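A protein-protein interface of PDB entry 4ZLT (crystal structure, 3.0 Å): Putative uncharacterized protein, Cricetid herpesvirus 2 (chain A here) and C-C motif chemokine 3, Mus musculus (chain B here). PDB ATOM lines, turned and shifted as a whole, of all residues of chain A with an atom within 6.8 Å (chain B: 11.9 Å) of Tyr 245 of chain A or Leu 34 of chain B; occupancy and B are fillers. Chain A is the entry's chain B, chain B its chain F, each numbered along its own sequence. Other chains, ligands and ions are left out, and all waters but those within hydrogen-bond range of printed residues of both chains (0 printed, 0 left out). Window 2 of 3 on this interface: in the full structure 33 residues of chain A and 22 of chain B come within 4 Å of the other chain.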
ATOM      1  N   GLU A 115      -7.401 -22.929 -20.872  1.00  0.00           N
ATOM      2  CA  GLU A 115      -6.538 -21.903 -21.423  1.00  0.00           C
ATOM      3  C   GLU A 115      -6.417 -22.070 -22.933  1.00  0.00           C
ATOM      4  O   GLU A 115      -6.859 -23.062 -23.512  1.00  0.00           O
ATOM      5  CB  GLU A 115      -5.159 -21.962 -20.774  1.00  0.00           C
ATOM      6  CG  GLU A 115      -5.143 -21.571 -19.322  1.00  0.00           C
ATOM      7  CD  GLU A 115      -3.745 -21.559 -18.759  1.00  0.00           C
ATOM      8  OE1 GLU A 115      -2.804 -21.906 -19.501  1.00  0.00           O
ATOM      9  OE2 GLU A 115      -3.587 -21.204 -17.576  1.00  0.00           O
ATOM     10  N   THR A 200      -7.923  -3.325 -13.854  1.00  0.00           N
ATOM     11  CA  THR A 200      -8.984  -3.999 -13.116  1.00  0.00           C
ATOM     12  C   THR A 200      -8.576  -5.416 -12.739  1.00  0.00           C
ATOM     13  O   THR A 200      -8.881  -5.884 -11.638  1.00  0.00           O
ATOM     14  CB  THR A 200     -10.270  -4.021 -13.940  1.00  0.00           C
ATOM     15  OG1 THR A 200     -10.755  -2.684 -14.112  1.00  0.00           O
ATOM     16  CG2 THR A 200     -11.330  -4.851 -13.241  1.00  0.00           C
ATOM     17  N   THR A 201      -7.883  -6.108 -13.636  1.00  0.00           N
ATOM     18  CA  THR A 201      -7.490  -7.493 -13.450  1.00  0.00           C
ATOM     19  C   THR A 201      -5.998  -7.588 -13.157  1.00  0.00           C
ATOM     20  O   THR A 201      -5.222  -6.672 -13.444  1.00  0.00           O
ATOM     21  CB  THR A 201      -7.832  -8.328 -14.689  1.00  0.00           C
ATOM     22  OG1 THR A 201      -9.231  -8.212 -14.969  1.00  0.00           O
ATOM     23  CG2 THR A 201      -7.499  -9.786 -14.465  1.00  0.00           C
ATOM     24  N   VAL A 202      -5.604  -8.722 -12.570  1.00  0.00           N
ATOM     25  CA  VAL A 202      -4.198  -8.993 -12.297  1.00  0.00           C
ATOM     26  C   VAL A 202      -3.517  -9.740 -13.436  1.00  0.00           C
ATOM     27  O   VAL A 202      -2.308 -10.000 -13.359  1.00  0.00           O
ATOM     28  CB  VAL A 202      -4.050  -9.788 -10.983  1.00  0.00           C
ATOM     29  CG1 VAL A 202      -2.604  -9.813 -10.539  1.00  0.00           C
ATOM     30  CG2 VAL A 202      -4.928  -9.187  -9.903  1.00  0.00           C
ATOM     31  N   LEU A 203      -4.250 -10.086 -14.493  1.00  0.00           N
ATOM     32  CA  LEU A 203      -3.667 -10.849 -15.589  1.00  0.00           C
ATOM     33  C   LEU A 203      -2.458 -10.125 -16.165  1.00  0.00           C
ATOM     34  O   LEU A 203      -2.470  -8.907 -16.345  1.00  0.00           O
ATOM     35  CB  LEU A 203      -4.704 -11.077 -16.687  1.00  0.00           C
ATOM     36  CG  LEU A 203      -5.965 -11.851 -16.308  1.00  0.00           C
ATOM     37  CD1 LEU A 203      -6.851 -12.043 -17.521  1.00  0.00           C
ATOM     38  CD2 LEU A 203      -5.596 -13.186 -15.699  1.00  0.00           C
ATOM     39  N   GLU A 204      -1.409 -10.885 -16.455  1.00  0.00           N
ATOM     40  CA  GLU A 204      -0.231 -10.309 -17.084  1.00  0.00           C
ATOM     41  C   GLU A 204      -0.561  -9.872 -18.505  1.00  0.00           C
ATOM     42  O   GLU A 204      -1.171 -10.623 -19.272  1.00  0.00           O
ATOM     43  CB  GLU A 204       0.919 -11.315 -17.090  1.00  0.00           C
ATOM     44  CG  GLU A 204       1.523 -11.588 -15.722  1.00  0.00           C
ATOM     45  CD  GLU A 204       2.779 -12.437 -15.802  1.00  0.00           C
ATOM     46  OE1 GLU A 204       3.166 -12.819 -16.927  1.00  0.00           O
ATOM     47  OE2 GLU A 204       3.381 -12.720 -14.745  1.00  0.00           O
ATOM     48  N   GLY A 243      -5.562 -11.962 -21.034  1.00  0.00           N
ATOM     49  CA  GLY A 243      -4.221 -11.938 -20.494  1.00  0.00           C
ATOM     50  C   GLY A 243      -3.790 -13.325 -20.087  1.00  0.00           C
ATOM     51  O   GLY A 243      -4.371 -14.321 -20.519  1.00  0.00           O
ATOM     52  N   PHE A 244      -2.767 -13.378 -19.244  1.00  0.00           N
ATOM     53  CA  PHE A 244      -2.189 -14.632 -18.794  1.00  0.00           C
ATOM     54  C   PHE A 244      -2.055 -14.619 -17.278  1.00  0.00           C
ATOM     55  O   PHE A 244      -1.826 -13.573 -16.670  1.00  0.00           O
ATOM     56  CB  PHE A 244      -0.814 -14.872 -19.429  1.00  0.00           C
ATOM     57  CG  PHE A 244      -0.783 -14.660 -20.912  1.00  0.00           C
ATOM     58  CD1 PHE A 244      -1.045 -15.702 -21.779  1.00  0.00           C
ATOM     59  CD2 PHE A 244      -0.481 -13.420 -21.439  1.00  0.00           C
ATOM     60  CE1 PHE A 244      -1.012 -15.510 -23.147  1.00  0.00           C
ATOM     61  CE2 PHE A 244      -0.446 -13.222 -22.807  1.00  0.00           C
ATOM     62  CZ  PHE A 244      -0.713 -14.270 -23.661  1.00  0.00           C
ATOM     63  N   TYR A 245      -2.198 -15.795 -16.675  1.00  0.00           N
ATOM     64  CA  TYR A 245      -1.963 -15.929 -15.246  1.00  0.00           C
ATOM     65  C   TYR A 245      -0.487 -15.714 -14.928  1.00  0.00           C
ATOM     66  O   TYR A 245       0.399 -16.074 -15.707  1.00  0.00           O
ATOM     67  CB  TYR A 245      -2.395 -17.312 -14.750  1.00  0.00           C
ATOM     68  CG  TYR A 245      -3.877 -17.602 -14.837  1.00  0.00           C
ATOM     69  CD1 TYR A 245      -4.781 -16.956 -14.011  1.00  0.00           C
ATOM     70  CD2 TYR A 245      -4.367 -18.550 -15.722  1.00  0.00           C
ATOM     71  CE1 TYR A 245      -6.132 -17.229 -14.081  1.00  0.00           C
ATOM     72  CE2 TYR A 245      -5.712 -18.831 -15.797  1.00  0.00           C
ATOM     73  CZ  TYR A 245      -6.591 -18.169 -14.975  1.00  0.00           C
ATOM     74  OH  TYR A 245      -7.937 -18.444 -15.049  1.00  0.00           O
ATOM     75  N   LYS A 246      -0.228 -15.121 -13.763  1.00  0.00           N
ATOM     76  CA  LYS A 246       1.143 -14.959 -13.299  1.00  0.00           C
ATOM     77  C   LYS A 246       1.861 -16.300 -13.303  1.00  0.00           C
ATOM     78  O   LYS A 246       1.245 -17.355 -13.132  1.00  0.00           O
ATOM     79  CB  LYS A 246       1.165 -14.370 -11.889  1.00  0.00           C
ATOM     80  CG  LYS A 246       0.578 -12.977 -11.763  1.00  0.00           C
ATOM     81  CD  LYS A 246       0.473 -12.589 -10.295  1.00  0.00           C
ATOM     82  CE  LYS A 246       0.193 -11.110 -10.112  1.00  0.00           C
ATOM     83  NZ  LYS A 246       0.063 -10.765  -8.668  1.00  0.00           N
ATOM     84  N   ARG A 247       3.177 -16.262 -13.496  1.00  0.00           N
ATOM     85  CA  ARG A 247       3.968 -17.484 -13.475  1.00  0.00           C
ATOM     86  C   ARG A 247       5.356 -17.195 -12.924  1.00  0.00           C
ATOM     87  O   ARG A 247       5.798 -16.045 -12.859  1.00  0.00           O
ATOM     88  CB  ARG A 247       4.057 -18.128 -14.863  1.00  0.00           C
ATOM     89  CG  ARG A 247       4.462 -17.206 -15.994  1.00  0.00           C
ATOM     90  CD  ARG A 247       4.557 -18.010 -17.275  1.00  0.00           C
ATOM     91  NE  ARG A 247       3.387 -18.868 -17.439  1.00  0.00           N
ATOM     92  CZ  ARG A 247       3.391 -20.025 -18.094  1.00  0.00           C
ATOM     93  NH1 ARG A 247       2.276 -20.737 -18.189  1.00  0.00           N
ATOM     94  NH2 ARG A 247       4.509 -20.478 -18.645  1.00  0.00           N
ATOM     95  N   GLY A 258      -0.452 -19.631 -22.758  1.00  0.00           N
ATOM     96  CA  GLY A 258      -1.842 -19.982 -22.542  1.00  0.00           C
ATOM     97  C   GLY A 258      -2.688 -18.823 -22.063  1.00  0.00           C
ATOM     98  O   GLY A 258      -2.662 -18.467 -20.883  1.00  0.00           O
ATOM     99  N   MET A 259      -3.454 -18.233 -22.972  1.00  0.00           N
ATOM    100  CA  MET A 259      -4.233 -17.046 -22.667  1.00  0.00           C
ATOM    101  C   MET A 259      -5.590 -17.422 -22.088  1.00  0.00           C
ATOM    102  O   MET A 259      -6.143 -18.483 -22.382  1.00  0.00           O
ATOM    103  CB  MET A 259      -4.419 -16.194 -23.924  1.00  0.00           C
ATOM    104  CG  MET A 259      -5.064 -14.843 -23.682  1.00  0.00           C
ATOM    105  SD  MET A 259      -5.260 -13.927 -25.217  1.00  0.00           S
ATOM    106  CE  MET A 259      -3.561 -13.859 -25.765  1.00  0.00           C
ATOM    107  N   VAL A 260      -6.123 -16.531 -21.255  1.00  0.00           N
ATOM    108  CA  VAL A 260      -7.440 -16.693 -20.655  1.00  0.00           C
ATOM    109  C   VAL A 260      -8.152 -15.349 -20.703  1.00  0.00           C
ATOM    110  O   VAL A 260      -7.570 -14.326 -21.067  1.00  0.00           O
ATOM    111  CB  VAL A 260      -7.365 -17.214 -19.206  1.00  0.00           C
ATOM    112  CG1 VAL A 260      -6.723 -18.582 -19.173  1.00  0.00           C
ATOM    113  CG2 VAL A 260      -6.590 -16.245 -18.338  1.00  0.00           C
ATOM    114  N   TYR A 261      -9.428 -15.358 -20.329  1.00  0.00           N
ATOM    115  CA  TYR A 261     -10.227 -14.146 -20.298  1.00  0.00           C
ATOM    116  C   TYR A 261     -10.912 -14.011 -18.946  1.00  0.00           C
ATOM    117  O   TYR A 261     -11.042 -14.976 -18.193  1.00  0.00           O
ATOM    118  CB  TYR A 261     -11.264 -14.124 -21.430  1.00  0.00           C
ATOM    119  CG  TYR A 261     -12.448 -15.045 -21.258  1.00  0.00           C
ATOM    120  CD1 TYR A 261     -13.539 -14.663 -20.499  1.00  0.00           C
ATOM    121  CD2 TYR A 261     -12.497 -16.274 -21.895  1.00  0.00           C
ATOM    122  CE1 TYR A 261     -14.628 -15.485 -20.353  1.00  0.00           C
ATOM    123  CE2 TYR A 261     -13.588 -17.106 -21.755  1.00  0.00           C
ATOM    124  CZ  TYR A 261     -14.650 -16.703 -20.981  1.00  0.00           C
ATOM    125  OH  TYR A 261     -15.745 -17.516 -20.827  1.00  0.00           O
ATOM    126  N   VAL A 262     -11.343 -12.788 -18.644  1.00  0.00           N
ATOM    127  CA  VAL A 262     -12.054 -12.478 -17.409  1.00  0.00           C
ATOM    128  C   VAL A 262     -13.171 -11.494 -17.725  1.00  0.00           C
ATOM    129  O   VAL A 262     -12.928 -10.431 -18.301  1.00  0.00           O
ATOM    130  CB  VAL A 262     -11.123 -11.893 -16.330  1.00  0.00           C
ATOM    131  CG1 VAL A 262     -11.912 -11.562 -15.084  1.00  0.00           C
ATOM    132  CG2 VAL A 262     -10.008 -12.861 -16.007  1.00  0.00           C
ATOM    133  N   THR B   8     -16.887 -19.670  -5.882  1.00  0.00           N
ATOM    134  CA  THR B   8     -17.403 -18.340  -6.187  1.00  0.00           C
ATOM    135  C   THR B   8     -17.283 -18.031  -7.676  1.00  0.00           C
ATOM    136  O   THR B   8     -16.278 -18.364  -8.304  1.00  0.00           O
ATOM    137  CB  THR B   8     -16.665 -17.254  -5.387  1.00  0.00           C
ATOM    138  OG1 THR B   8     -15.254 -17.373  -5.608  1.00  0.00           O
ATOM    139  CG2 THR B   8     -16.957 -17.395  -3.901  1.00  0.00           C
ATOM    140  N   PRO B   9     -18.312 -17.400  -8.240  1.00  0.00           N
ATOM    141  CA  PRO B   9     -18.254 -17.023  -9.658  1.00  0.00           C
ATOM    142  C   PRO B   9     -17.117 -16.048  -9.935  1.00  0.00           C
ATOM    143  O   PRO B   9     -16.889 -15.094  -9.186  1.00  0.00           O
ATOM    144  CB  PRO B   9     -19.623 -16.380  -9.910  1.00  0.00           C
ATOM    145  CG  PRO B   9     -20.509 -16.948  -8.843  1.00  0.00           C
ATOM    146  CD  PRO B   9     -19.627 -17.114  -7.642  1.00  0.00           C
ATOM    147  N   THR B  10     -16.405 -16.298 -11.032  1.00  0.00           N
ATOM    148  CA  THR B  10     -15.238 -15.509 -11.421  1.00  0.00           C
ATOM    149  C   THR B  10     -15.688 -14.324 -12.270  1.00  0.00           C
ATOM    150  O   THR B  10     -16.149 -14.500 -13.404  1.00  0.00           O
ATOM    151  CB  THR B  10     -14.231 -16.371 -12.177  1.00  0.00           C
ATOM    152  OG1 THR B  10     -14.863 -16.949 -13.325  1.00  0.00           O
ATOM    153  CG2 THR B  10     -13.699 -17.477 -11.278  1.00  0.00           C
ATOM    154  N   ALA B  11     -15.553 -13.119 -11.723  1.00  0.00           N
ATOM    155  CA  ALA B  11     -15.885 -11.898 -12.442  1.00  0.00           C
ATOM    156  C   ALA B  11     -15.242 -10.727 -11.718  1.00  0.00           C
ATOM    157  O   ALA B  11     -14.970 -10.804 -10.518  1.00  0.00           O
ATOM    158  CB  ALA B  11     -17.400 -11.699 -12.550  1.00  0.00           C
ATOM    159  N   CYS B  12     -14.985  -9.650 -12.461  1.00  0.00           N
ATOM    160  CA  CYS B  12     -14.345  -8.466 -11.908  1.00  0.00           C
ATOM    161  C   CYS B  12     -15.191  -7.231 -12.176  1.00  0.00           C
ATOM    162  O   CYS B  12     -15.897  -7.146 -13.181  1.00  0.00           O
ATOM    163  CB  CYS B  12     -12.942  -8.269 -12.478  1.00  0.00           C
ATOM    164  SG  CYS B  12     -11.778  -9.499 -11.901  1.00  0.00           S
ATOM    165  N   CYS B  13     -15.111  -6.276 -11.253  1.00  0.00           N
ATOM    166  CA  CYS B  13     -15.855  -5.023 -11.343  1.00  0.00           C
ATOM    167  C   CYS B  13     -15.048  -3.981 -12.111  1.00  0.00           C
ATOM    168  O   CYS B  13     -14.021  -3.501 -11.624  1.00  0.00           O
ATOM    169  CB  CYS B  13     -16.201  -4.513  -9.949  1.00  0.00           C
ATOM    170  SG  CYS B  13     -17.437  -5.501  -9.119  1.00  0.00           S
ATOM    171  N   PHE B  14     -15.515  -3.626 -13.308  1.00  0.00           N
ATOM    172  CA  PHE B  14     -14.881  -2.564 -14.080  1.00  0.00           C
ATOM    173  C   PHE B  14     -15.346  -1.176 -13.665  1.00  0.00           C
ATOM    174  O   PHE B  14     -14.619  -0.200 -13.881  1.00  0.00           O
ATOM    175  CB  PHE B  14     -15.158  -2.760 -15.571  1.00  0.00           C
ATOM    176  CG  PHE B  14     -14.298  -1.913 -16.462  1.00  0.00           C
ATOM    177  CD1 PHE B  14     -13.003  -2.289 -16.763  1.00  0.00           C
ATOM    178  CD2 PHE B  14     -14.788  -0.735 -16.996  1.00  0.00           C
ATOM    179  CE1 PHE B  14     -12.216  -1.504 -17.582  1.00  0.00           C
ATOM    180  CE2 PHE B  14     -14.006   0.049 -17.813  1.00  0.00           C
ATOM    181  CZ  PHE B  14     -12.721  -0.336 -18.106  1.00  0.00           C
ATOM    182  N   TYR B  16     -18.284   0.757 -10.598  1.00  0.00           N
ATOM    183  CA  TYR B  16     -19.239   0.518  -9.530  1.00  0.00           C
ATOM    184  C   TYR B  16     -20.559   1.225  -9.812  1.00  0.00           C
ATOM    185  O   TYR B  16     -20.640   2.146 -10.625  1.00  0.00           O
ATOM    186  CB  TYR B  16     -18.654   0.970  -8.195  1.00  0.00           C
ATOM    187  CG  TYR B  16     -17.375   0.242  -7.855  1.00  0.00           C
ATOM    188  CD1 TYR B  16     -17.358  -1.136  -7.702  1.00  0.00           C
ATOM    189  CD2 TYR B  16     -16.182   0.929  -7.698  1.00  0.00           C
ATOM    190  CE1 TYR B  16     -16.194  -1.808  -7.398  1.00  0.00           C
ATOM    191  CE2 TYR B  16     -15.012   0.266  -7.393  1.00  0.00           C
ATOM    192  CZ  TYR B  16     -15.024  -1.103  -7.244  1.00  0.00           C
ATOM    193  OH  TYR B  16     -13.859  -1.769  -6.938  1.00  0.00           O
ATOM    194  N   PHE B  29     -21.802 -11.439  -3.014  1.00  0.00           N
ATOM    195  CA  PHE B  29     -20.583 -12.211  -2.810  1.00  0.00           C
ATOM    196  C   PHE B  29     -19.398 -11.388  -3.284  1.00  0.00           C
ATOM    197  O   PHE B  29     -19.514 -10.597  -4.221  1.00  0.00           O
ATOM    198  CB  PHE B  29     -20.623 -13.559  -3.538  1.00  0.00           C
ATOM    199  CG  PHE B  29     -20.839 -13.449  -5.017  1.00  0.00           C
ATOM    200  CD1 PHE B  29     -19.766 -13.267  -5.870  1.00  0.00           C
ATOM    201  CD2 PHE B  29     -22.108 -13.553  -5.554  1.00  0.00           C
ATOM    202  CE1 PHE B  29     -19.956 -13.176  -7.232  1.00  0.00           C
ATOM    203  CE2 PHE B  29     -22.305 -13.463  -6.915  1.00  0.00           C
ATOM    204  CZ  PHE B  29     -21.227 -13.274  -7.756  1.00  0.00           C
ATOM    205  N   GLU B  30     -18.261 -11.582  -2.623  1.00  0.00           N
ATOM    206  CA  GLU B  30     -17.065 -10.823  -2.949  1.00  0.00           C
ATOM    207  C   GLU B  30     -16.479 -11.305  -4.274  1.00  0.00           C
ATOM    208  O   GLU B  30     -16.710 -12.436  -4.712  1.00  0.00           O
ATOM    209  CB  GLU B  30     -16.038 -10.946  -1.824  1.00  0.00           C
ATOM    210  CG  GLU B  30     -16.590 -10.564  -0.456  1.00  0.00           C
ATOM    211  CD  GLU B  30     -15.655 -10.929   0.684  1.00  0.00           C
ATOM    212  OE1 GLU B  30     -14.493 -11.296   0.411  1.00  0.00           O
ATOM    213  OE2 GLU B  30     -16.090 -10.860   1.853  1.00  0.00           O
ATOM    214  N   THR B  31     -15.710 -10.429  -4.914  1.00  0.00           N
ATOM    215  CA  THR B  31     -15.155 -10.741  -6.221  1.00  0.00           C
ATOM    216  C   THR B  31     -13.940 -11.655  -6.109  1.00  0.00           C
ATOM    217  O   THR B  31     -13.310 -11.778  -5.056  1.00  0.00           O
ATOM    218  CB  THR B  31     -14.768  -9.465  -6.968  1.00  0.00           C
ATOM    219  OG1 THR B  31     -13.808  -8.731  -6.201  1.00  0.00           O
ATOM    220  CG2 THR B  31     -15.991  -8.599  -7.205  1.00  0.00           C
ATOM    221  N   SER B  32     -13.607 -12.282  -7.234  1.00  0.00           N
ATOM    222  CA  SER B  32     -12.501 -13.223  -7.295  1.00  0.00           C
ATOM    223  C   SER B  32     -11.187 -12.552  -6.909  1.00  0.00           C
ATOM    224  O   SER B  32     -11.067 -11.326  -6.869  1.00  0.00           O
ATOM    225  CB  SER B  32     -12.386 -13.818  -8.696  1.00  0.00           C
ATOM    226  OG  SER B  32     -11.212 -14.600  -8.815  1.00  0.00           O
ATOM    227  N   SER B  33     -10.191 -13.386  -6.612  1.00  0.00           N
ATOM    228  CA  SER B  33      -8.850 -12.897  -6.328  1.00  0.00           C
ATOM    229  C   SER B  33      -8.109 -12.455  -7.582  1.00  0.00           C
ATOM    230  O   SER B  33      -7.019 -11.886  -7.466  1.00  0.00           O
ATOM    231  CB  SER B  33      -8.042 -13.975  -5.607  1.00  0.00           C
ATOM    232  OG  SER B  33      -8.026 -15.180  -6.354  1.00  0.00           O
ATOM    233  N   LEU B  34      -8.659 -12.716  -8.770  1.00  0.00           N
ATOM    234  CA  LEU B  34      -8.048 -12.224  -9.999  1.00  0.00           C
ATOM    235  C   LEU B  34      -8.239 -10.723 -10.174  1.00  0.00           C
ATOM    236  O   LEU B  34      -7.486 -10.097 -10.926  1.00  0.00           O
ATOM    237  CB  LEU B  34      -8.628 -12.969 -11.204  1.00  0.00           C
ATOM    238  CG  LEU B  34      -8.284 -14.456 -11.323  1.00  0.00           C
ATOM    239  CD1 LEU B  34      -8.986 -15.079 -12.513  1.00  0.00           C
ATOM    240  CD2 LEU B  34      -6.783 -14.643 -11.442  1.00  0.00           C
ATOM    241  N   CYS B  35      -9.226 -10.142  -9.500  1.00  0.00           N
ATOM    242  CA  CYS B  35      -9.522  -8.724  -9.630  1.00  0.00           C
ATOM    243  C   CYS B  35      -8.543  -7.905  -8.799  1.00  0.00           C
ATOM    244  O   CYS B  35      -8.303  -8.212  -7.627  1.00  0.00           O
ATOM    245  CB  CYS B  35     -10.954  -8.451  -9.183  1.00  0.00           C
ATOM    246  SG  CYS B  35     -12.160  -9.561  -9.918  1.00  0.00           S
ATOM    247  N   SER B  36      -7.975  -6.861  -9.404  1.00  0.00           N
ATOM    248  CA  SER B  36      -7.014  -6.033  -8.684  1.00  0.00           C
ATOM    249  C   SER B  36      -7.666  -5.314  -7.510  1.00  0.00           C
ATOM    250  O   SER B  36      -7.056  -5.175  -6.443  1.00  0.00           O
ATOM    251  CB  SER B  36      -6.371  -5.025  -9.636  1.00  0.00           C
ATOM    252  OG  SER B  36      -7.257  -3.957  -9.920  1.00  0.00           O
ATOM    253  N   GLN B  37      -8.901  -4.851  -7.683  1.00  0.00           N
ATOM    254  CA  GLN B  37      -9.581  -4.096  -6.642  1.00  0.00           C
ATOM    255  C   GLN B  37     -10.693  -4.926  -6.025  1.00  0.00           C
ATOM    256  O   GLN B  37     -11.489  -5.529  -6.759  1.00  0.00           O
ATOM    257  CB  GLN B  37     -10.155  -2.794  -7.209  1.00  0.00           C
ATOM    258  CG  GLN B  37     -10.311  -1.694  -6.175  1.00  0.00           C
ATOM    259  CD  GLN B  37      -8.976  -1.171  -5.685  1.00  0.00           C
ATOM    260  OE1 GLN B  37      -7.924  -1.520  -6.222  1.00  0.00           O
ATOM    261  NE2 GLN B  37      -9.010  -0.331  -4.658  1.00  0.00           N
ATOM    262  N   PRO B  38     -10.784  -4.988  -4.696  1.00  0.00           N
ATOM    263  CA  PRO B  38     -11.851  -5.770  -4.053  1.00  0.00           C
ATOM    264  C   PRO B  38     -13.209  -5.116  -4.263  1.00  0.00           C
ATOM    265  O   PRO B  38     -13.439  -3.982  -3.837  1.00  0.00           O
ATOM    266  CB  PRO B  38     -11.445  -5.767  -2.577  1.00  0.00           C
ATOM    267  CG  PRO B  38     -10.697  -4.483  -2.424  1.00  0.00           C
ATOM    268  CD  PRO B  38      -9.916  -4.333  -3.703  1.00  0.00           C
ATOM    269  N   GLY B  39     -14.110  -5.842  -4.921  1.00  0.00           N
ATOM    270  CA  GLY B  39     -15.433  -5.337  -5.197  1.00  0.00           C
ATOM    271  C   GLY B  39     -16.495  -6.313  -4.731  1.00  0.00           C
ATOM    272  O   GLY B  39     -16.231  -7.487  -4.482  1.00  0.00           O
ATOM    273  N   ILE B  41     -20.356  -7.899  -5.582  1.00  0.00           N
ATOM    274  CA  ILE B  41     -21.290  -8.179  -6.662  1.00  0.00           C
ATOM    275  C   ILE B  41     -22.623  -8.534  -6.027  1.00  0.00           C
ATOM    276  O   ILE B  41     -22.779  -9.627  -5.469  1.00  0.00           O
ATOM    277  CB  ILE B  41     -20.795  -9.306  -7.573  1.00  0.00           C
ATOM    278  CG1 ILE B  41     -19.412  -8.971  -8.127  1.00  0.00           C
ATOM    279  CG2 ILE B  41     -21.783  -9.551  -8.700  1.00  0.00           C
ATOM    280  CD1 ILE B  41     -18.855 -10.028  -9.037  1.00  0.00           C
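The backbone NH (N) of Ser 36 of chain B lies within hydrogen-bond range of the backbone carbonyl oxygen (O) of Thr 200 of chain A (2.6 Å).
N of Val 202 of chain A is in hydrogen-bond range of O of Leu 34 of chain B, at 2.9 Å.
The side-chain sulfur of Cys 12 of chain B forms a disulfide with the side-chain sulfur of Cys 35 of chain B (2.0 Å).
OG of Ser 32 of chain B lies close to N of Leu 34 of chain B (3.2 Å).
Among the printed residues, merely in contact across the chains: Thr 200 of chain A with Cys 12 of chain B (3.9 Å), Thr 200 of chain A with Cys 13 of chain B (3.4 Å), Thr 200 of chain A with Phe 14 of chain B (3.5 Å), Thr 200 of chain A with Cys 35 of chain B (3.5 Å), Thr 201 of chain A with Leu 34 of chain B (3.6 Å), Val 202 of chain A with Cys 35 of chain B (3.99 Å), Val 202 of chain A with Ser 36 of chain B (3.9 Å), Tyr 245 of chain A with Leu 34 of chain B (3.8 Å) and Val 262 of chain A with Cys 12 of chain B (3.8 Å).
Tyr 245 of chain A touches just one residue of chain B: Leu 34.
Leu 34 of chain B touches just these residues of chain A: Thr 201, Val 202 and Tyr 245.
Thr 201 of chain A touches just one residue of chain B: Leu 34 (3.6 Å).
No residue of chain B comes within 4 Å of Arg 247 of chain A.
No residue of chain B comes within 4 Å of Val 260 of chain A.
Of the printed residues of chain A, Cys 12 of chain B touches Thr 200 (3.9 Å) and Val 262 (3.8 Å).
Of the printed residues of chain B, Thr 200 of chain A touches Cys 12, Cys 13, Phe 14, Cys 35 and Ser 36.
Of the printed residues of chain A, Cys 13 of chain B touches Thr 200 (3.4 Å).
Thr 8 of chain B touches none of the printed residues of chain A.
Thr 10 of chain B touches none of the printed residues of chain A.
The nearest residue of chain B that does not touch Tyr 245 of chain A is Thr 10 of chain B (7.0 Å).
Along chain A the printed residues that touch a printed residue of chain B span positions 200 to 262.
Hydrophobic or aromatic side chains of chain B that line the printed part of chain A: Phe 14 and Leu 34.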
